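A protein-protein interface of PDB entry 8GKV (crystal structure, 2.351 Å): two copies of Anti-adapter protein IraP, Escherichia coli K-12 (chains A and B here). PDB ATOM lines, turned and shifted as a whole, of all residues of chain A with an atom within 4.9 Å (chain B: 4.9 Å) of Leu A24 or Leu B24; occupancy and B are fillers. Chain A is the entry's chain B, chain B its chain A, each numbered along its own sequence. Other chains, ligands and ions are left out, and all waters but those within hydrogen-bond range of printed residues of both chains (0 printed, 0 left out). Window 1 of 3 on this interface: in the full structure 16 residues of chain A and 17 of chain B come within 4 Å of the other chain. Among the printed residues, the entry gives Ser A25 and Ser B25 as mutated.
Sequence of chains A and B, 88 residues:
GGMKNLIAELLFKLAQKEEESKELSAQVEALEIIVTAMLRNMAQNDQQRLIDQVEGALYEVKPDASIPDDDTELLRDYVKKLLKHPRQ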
ATOM      1  N   GLU A  20      19.044  33.391  15.849  1.00  0.00           N
ATOM      2  CA  GLU A  20      18.530  32.041  15.618  1.00  0.00           C
ATOM      3  C   GLU A  20      17.061  31.933  16.041  1.00  0.00           C
ATOM      4  O   GLU A  20      16.215  31.460  15.272  1.00  0.00           O
ATOM      5  CB  GLU A  20      19.376  31.008  16.367  1.00  0.00           C
ATOM      6  CG  GLU A  20      18.876  29.580  16.230  1.00  0.00           C
ATOM      7  CD  GLU A  20      19.774  28.582  16.937  1.00  0.00           C
ATOM      8  OE1 GLU A  20      20.560  29.004  17.810  1.00  0.00           O
ATOM      9  OE2 GLU A  20      19.697  27.376  16.619  1.00  0.00           O
ATOM     10  N   SER A  21      16.761  32.372  17.262  1.00  0.00           N
ATOM     11  CA  SER A  21      15.388  32.344  17.761  1.00  0.00           C
ATOM     12  C   SER A  21      14.453  33.139  16.852  1.00  0.00           C
ATOM     13  O   SER A  21      13.347  32.688  16.554  1.00  0.00           O
ATOM     14  CB  SER A  21      15.317  32.889  19.192  1.00  0.00           C
ATOM     15  OG  SER A  21      15.743  31.915  20.129  1.00  0.00           O
ATOM     16  N   LYS A  22      14.893  34.318  16.413  1.00  0.00           N
ATOM     17  CA  LYS A  22      14.114  35.111  15.458  1.00  0.00           C
ATOM     18  C   LYS A  22      13.766  34.278  14.206  1.00  0.00           C
ATOM     19  O   LYS A  22      12.572  34.094  13.860  1.00  0.00           O
ATOM     20  CB  LYS A  22      14.888  36.381  15.079  1.00  0.00           C
ATOM     21  CG  LYS A  22      14.179  37.311  14.105  1.00  0.00           C
ATOM     22  CD  LYS A  22      13.921  38.676  14.732  1.00  0.00           C
ATOM     23  CE  LYS A  22      13.462  39.688  13.691  1.00  0.00           C
ATOM     24  NZ  LYS A  22      13.089  41.006  14.285  1.00  0.00           N
ATOM     25  N   GLU A  23      14.801  33.755  13.547  1.00  0.00           N
ATOM     26  CA  GLU A  23      14.590  32.909  12.365  1.00  0.00           C
ATOM     27  C   GLU A  23      13.605  31.758  12.638  1.00  0.00           C
ATOM     28  O   GLU A  23      12.617  31.567  11.905  1.00  0.00           O
ATOM     29  CB  GLU A  23      15.924  32.341  11.868  1.00  0.00           C
ATOM     30  CG  GLU A  23      16.595  33.165  10.781  1.00  0.00           C
ATOM     31  CD  GLU A  23      18.062  33.430  11.061  1.00  0.00           C
ATOM     32  OE1 GLU A  23      18.811  32.459  11.305  1.00  0.00           O
ATOM     33  OE2 GLU A  23      18.466  34.613  11.040  1.00  0.00           O
ATOM     34  N   LEU A  24      13.870  30.999  13.700  1.00  0.00           N
ATOM     35  CA  LEU A  24      13.021  29.861  14.051  1.00  0.00           C
ATOM     36  C   LEU A  24      11.566  30.284  14.269  1.00  0.00           C
ATOM     37  O   LEU A  24      10.645  29.643  13.754  1.00  0.00           O
ATOM     38  CB  LEU A  24      13.572  29.161  15.295  1.00  0.00           C
ATOM     39  CG  LEU A  24      14.940  28.506  15.080  1.00  0.00           C
ATOM     40  CD1 LEU A  24      15.522  28.055  16.410  1.00  0.00           C
ATOM     41  CD2 LEU A  24      14.842  27.334  14.108  1.00  0.00           C
ATOM     42  N   SER A  25      11.366  31.362  15.021  1.00  0.00           N
ATOM     43  CA  SER A  25      10.031  31.895  15.252  1.00  0.00           C
ATOM     44  C   SER A  25       9.337  32.201  13.929  1.00  0.00           C
ATOM     45  O   SER A  25       8.164  31.848  13.731  1.00  0.00           O
ATOM     46  CB  SER A  25      10.103  33.160  16.104  1.00  0.00           C
ATOM     47  OG  SER A  25       8.823  33.529  16.581  1.00  0.00           O
ATOM     48  N   ALA A  26      10.054  32.867  13.034  1.00  0.00           N
ATOM     49  CA  ALA A  26       9.537  33.135  11.687  1.00  0.00           C
ATOM     50  C   ALA A  26       9.084  31.830  11.010  1.00  0.00           C
ATOM     51  O   ALA A  26       7.963  31.727  10.475  1.00  0.00           O
ATOM     52  CB  ALA A  26      10.579  33.844  10.839  1.00  0.00           C
ATOM     53  N   GLN A  27       9.961  30.826  11.048  1.00  0.00           N
ATOM     54  CA  GLN A  27       9.610  29.508  10.503  1.00  0.00           C
ATOM     55  C   GLN A  27       8.347  28.910  11.133  1.00  0.00           C
ATOM     56  O   GLN A  27       7.477  28.407  10.416  1.00  0.00           O
ATOM     57  CB  GLN A  27      10.768  28.526  10.669  1.00  0.00           C
ATOM     58  CG  GLN A  27      11.994  28.896   9.858  1.00  0.00           C
ATOM     59  CD  GLN A  27      13.064  27.825   9.875  1.00  0.00           C
ATOM     60  OE1 GLN A  27      12.775  26.634   9.765  1.00  0.00           O
ATOM     61  NE2 GLN A  27      14.315  28.249  10.009  1.00  0.00           N
ATOM     62  N   VAL A  28       8.242  28.951  12.459  1.00  0.00           N
ATOM     63  CA  VAL A  28       7.055  28.415  13.126  1.00  0.00           C
ATOM     64  C   VAL A  28       5.809  29.166  12.651  1.00  0.00           C
ATOM     65  O   VAL A  28       4.779  28.547  12.364  1.00  0.00           O
ATOM     66  CB  VAL A  28       7.169  28.493  14.666  1.00  0.00           C
ATOM     67  CG1 VAL A  28       5.858  28.067  15.341  1.00  0.00           C
ATOM     68  CG2 VAL A  28       8.315  27.621  15.145  1.00  0.00           C
ATOM     69  N   GLU B  20      14.707  28.460  24.824  1.00  0.00           N
ATOM     70  CA  GLU B  20      13.691  28.958  23.896  1.00  0.00           C
ATOM     71  C   GLU B  20      13.961  28.464  22.471  1.00  0.00           C
ATOM     72  O   GLU B  20      13.048  28.013  21.762  1.00  0.00           O
ATOM     73  CB  GLU B  20      13.659  30.492  23.951  1.00  0.00           C
ATOM     74  CG  GLU B  20      12.922  31.189  22.812  1.00  0.00           C
ATOM     75  CD  GLU B  20      13.096  32.702  22.853  1.00  0.00           C
ATOM     76  OE1 GLU B  20      13.461  33.231  23.926  1.00  0.00           O
ATOM     77  OE2 GLU B  20      12.879  33.363  21.815  1.00  0.00           O
ATOM     78  N   SER B  21      15.224  28.543  22.062  1.00  0.00           N
ATOM     79  CA  SER B  21      15.623  28.125  20.725  1.00  0.00           C
ATOM     80  C   SER B  21      15.402  26.630  20.534  1.00  0.00           C
ATOM     81  O   SER B  21      14.870  26.202  19.509  1.00  0.00           O
ATOM     82  CB  SER B  21      17.087  28.477  20.466  1.00  0.00           C
ATOM     83  OG  SER B  21      17.450  28.159  19.135  1.00  0.00           O
ATOM     84  N   LYS B  22      15.821  25.830  21.511  1.00  0.00           N
ATOM     85  CA  LYS B  22      15.591  24.386  21.415  1.00  0.00           C
ATOM     86  C   LYS B  22      14.088  24.063  21.302  1.00  0.00           C
ATOM     87  O   LYS B  22      13.669  23.248  20.454  1.00  0.00           O
ATOM     88  CB  LYS B  22      16.227  23.665  22.610  1.00  0.00           C
ATOM     89  CG  LYS B  22      17.759  23.685  22.588  1.00  0.00           C
ATOM     90  CD  LYS B  22      18.335  22.950  21.367  1.00  0.00           C
ATOM     91  CE  LYS B  22      19.440  23.748  20.673  1.00  0.00           C
ATOM     92  NZ  LYS B  22      18.960  25.028  20.065  1.00  0.00           N
ATOM     93  N   GLU B  23      13.271  24.716  22.128  1.00  0.00           N
ATOM     94  CA  GLU B  23      11.817  24.541  22.015  1.00  0.00           C
ATOM     95  C   GLU B  23      11.300  24.906  20.611  1.00  0.00           C
ATOM     96  O   GLU B  23      10.577  24.120  19.971  1.00  0.00           O
ATOM     97  CB  GLU B  23      11.092  25.375  23.071  1.00  0.00           C
ATOM     98  CG  GLU B  23      11.360  24.906  24.488  1.00  0.00           C
ATOM     99  CD  GLU B  23      10.637  25.739  25.531  1.00  0.00           C
ATOM    100  OE1 GLU B  23       9.494  26.172  25.265  1.00  0.00           O
ATOM    101  OE2 GLU B  23      11.212  25.969  26.616  1.00  0.00           O
ATOM    102  N   LEU B  24      11.674  26.088  20.126  1.00  0.00           N
ATOM    103  CA  LEU B  24      11.267  26.506  18.785  1.00  0.00           C
ATOM    104  C   LEU B  24      11.709  25.507  17.710  1.00  0.00           C
ATOM    105  O   LEU B  24      10.945  25.190  16.795  1.00  0.00           O
ATOM    106  CB  LEU B  24      11.816  27.893  18.465  1.00  0.00           C
ATOM    107  CG  LEU B  24      11.116  29.043  19.195  1.00  0.00           C
ATOM    108  CD1 LEU B  24      11.933  30.327  19.113  1.00  0.00           C
ATOM    109  CD2 LEU B  24       9.711  29.260  18.642  1.00  0.00           C
ATOM    110  N   SER B  25      12.945  25.023  17.824  1.00  0.00           N
ATOM    111  CA  SER B  25      13.463  24.009  16.908  1.00  0.00           C
ATOM    112  C   SER B  25      12.560  22.777  16.917  1.00  0.00           C
ATOM    113  O   SER B  25      12.144  22.285  15.857  1.00  0.00           O
ATOM    114  CB  SER B  25      14.898  23.627  17.285  1.00  0.00           C
ATOM    115  OG  SER B  25      15.761  24.747  17.189  1.00  0.00           O
ATOM    116  N   ALA B  26      12.252  22.288  18.120  1.00  0.00           N
ATOM    117  CA  ALA B  26      11.338  21.154  18.274  1.00  0.00           C
ATOM    118  C   ALA B  26      10.007  21.420  17.557  1.00  0.00           C
ATOM    119  O   ALA B  26       9.517  20.578  16.785  1.00  0.00           O
ATOM    120  CB  ALA B  26      11.094  20.860  19.746  1.00  0.00           C
ATOM    121  N   GLN B  27       9.426  22.592  17.811  1.00  0.00           N
ATOM    122  CA  GLN B  27       8.185  22.972  17.124  1.00  0.00           C
ATOM    123  C   GLN B  27       8.317  22.946  15.596  1.00  0.00           C
ATOM    124  O   GLN B  27       7.465  22.382  14.898  1.00  0.00           O
ATOM    125  CB  GLN B  27       7.730  24.364  17.560  1.00  0.00           C
ATOM    126  CG  GLN B  27       6.998  24.393  18.889  1.00  0.00           C
ATOM    127  CD  GLN B  27       6.819  25.800  19.422  1.00  0.00           C
ATOM    128  OE1 GLN B  27       6.867  26.772  18.668  1.00  0.00           O
ATOM    129  NE2 GLN B  27       6.618  25.917  20.730  1.00  0.00           N
ATOM    130  N   VAL B  28       9.374  23.566  15.079  1.00  0.00           N
ATOM    131  CA  VAL B  28       9.613  23.585  13.638  1.00  0.00           C
ATOM    132  C   VAL B  28       9.660  22.162  13.092  1.00  0.00           C
ATOM    133  O   VAL B  28       9.016  21.849  12.082  1.00  0.00           O
ATOM    134  CB  VAL B  28      10.926  24.333  13.287  1.00  0.00           C
ATOM    135  CG1 VAL B  28      11.368  24.037  11.857  1.00  0.00           C
ATOM    136  CG2 VAL B  28      10.739  25.826  13.480  1.00  0.00           C
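The backbone carbonyl oxygen of Ser B21 lies within hydrogen-bond range of the side-chain hydroxyl of Ser B25, at 2.9 Å.
Among the printed residues, merely in contact across the chains: Ser A21 with Glu B20 (3.6 Å), Ser A21 with Ser B21 (3.7 Å), Ser A21 with Leu B24 (3.8 Å), Leu A24 with Ser B21 (3.3 Å), Leu A24 with Leu B24 (3.8 Å), Leu A24 with Ser B25 (3.4 Å), Leu A24 with Val B28 (3.8 Å), Gln A27 with Val B28 (3.6 Å), Val A28 with Leu B24 (3.9 Å), Val A28 with Gln B27 (3.7 Å) and Val A28 with Val B28 (3.4 Å).
Of the 9 printed residues of chain A, 5 touch a printed residue of chain B. Printed residues of chain A that touch a printed residue of chain B: Glu A20, Ser A21, Leu A24, Gln A27 and Val A28. Printed residues of chain B that touch a printed residue of chain A: Glu B20, Ser B21, Leu B24, Ser B25, Gln B27 and Val B28. Hydrophobic or aromatic side chains of chain B that line the printed part of chain A: Leu B24 and Val B28. Among the printed residues, no Asp or Glu carboxylate lies within 4 Å of a Lys or Arg side-chain nitrogen of the other chain.
Of the printed residues of chain B, Leu A24 touches Ser B21 (3.3 Å), Leu B24 (3.8 Å), Ser B25 (3.4 Å) and Val B28 (3.8 Å). Printed residues of chain A within 4 Å of Leu B24: Ser A21, Leu A24 and Val A28. Of the printed residues of chain A, Gln B27 touches Val A28. Printed residues of chain B within 4 Å of Ser A21: Glu B20, Ser B21 and Leu B24. Of the printed residues of chain A, Ser B21 touches Glu A20 (3.2 Å), Ser A21 (3.7 Å) and Leu A24 (3.3 Å). Of the printed residues of chain A, Glu B20 touches Ser A21 (3.6 Å). Of the printed residues of chain B, Val A28 touches Leu B24 (3.9 Å), Gln B27 (3.7 Å) and Val B28 (3.4 Å). Ala B26 touches none of the printed residues of chain A. Glu A23 touches none of the printed residues of chain B. The nearest printed residue of chain B that does not touch Leu A24 is Lys B22 (5.6 Å). The nearest printed residue of chain A that does not touch Leu B24 is Ser A25 (4.3 Å).
Glu A20 touches Ser B21, and with the chains exchanged Ser A21 touches Glu B20. Ser A21 touches its own counterpart, Ser B21. Ser A21 touches Leu B24, and with the chains exchanged Leu A24 touches Ser B21. Leu A24 touches Ser B25, but with the chains exchanged Ser A25 does not touch Leu B24 (4.3 Å). Positions printed for both chains: 20, 21, 22, 23, 24, 25, 26, 27 and 28. Of the 12 pairs that touch across the chains among the printed residues, 11 have their exchanged pair printed and touching as well.
OG of Ser B21 lies close to OE2 of Glu A20, 3.5 Å away.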
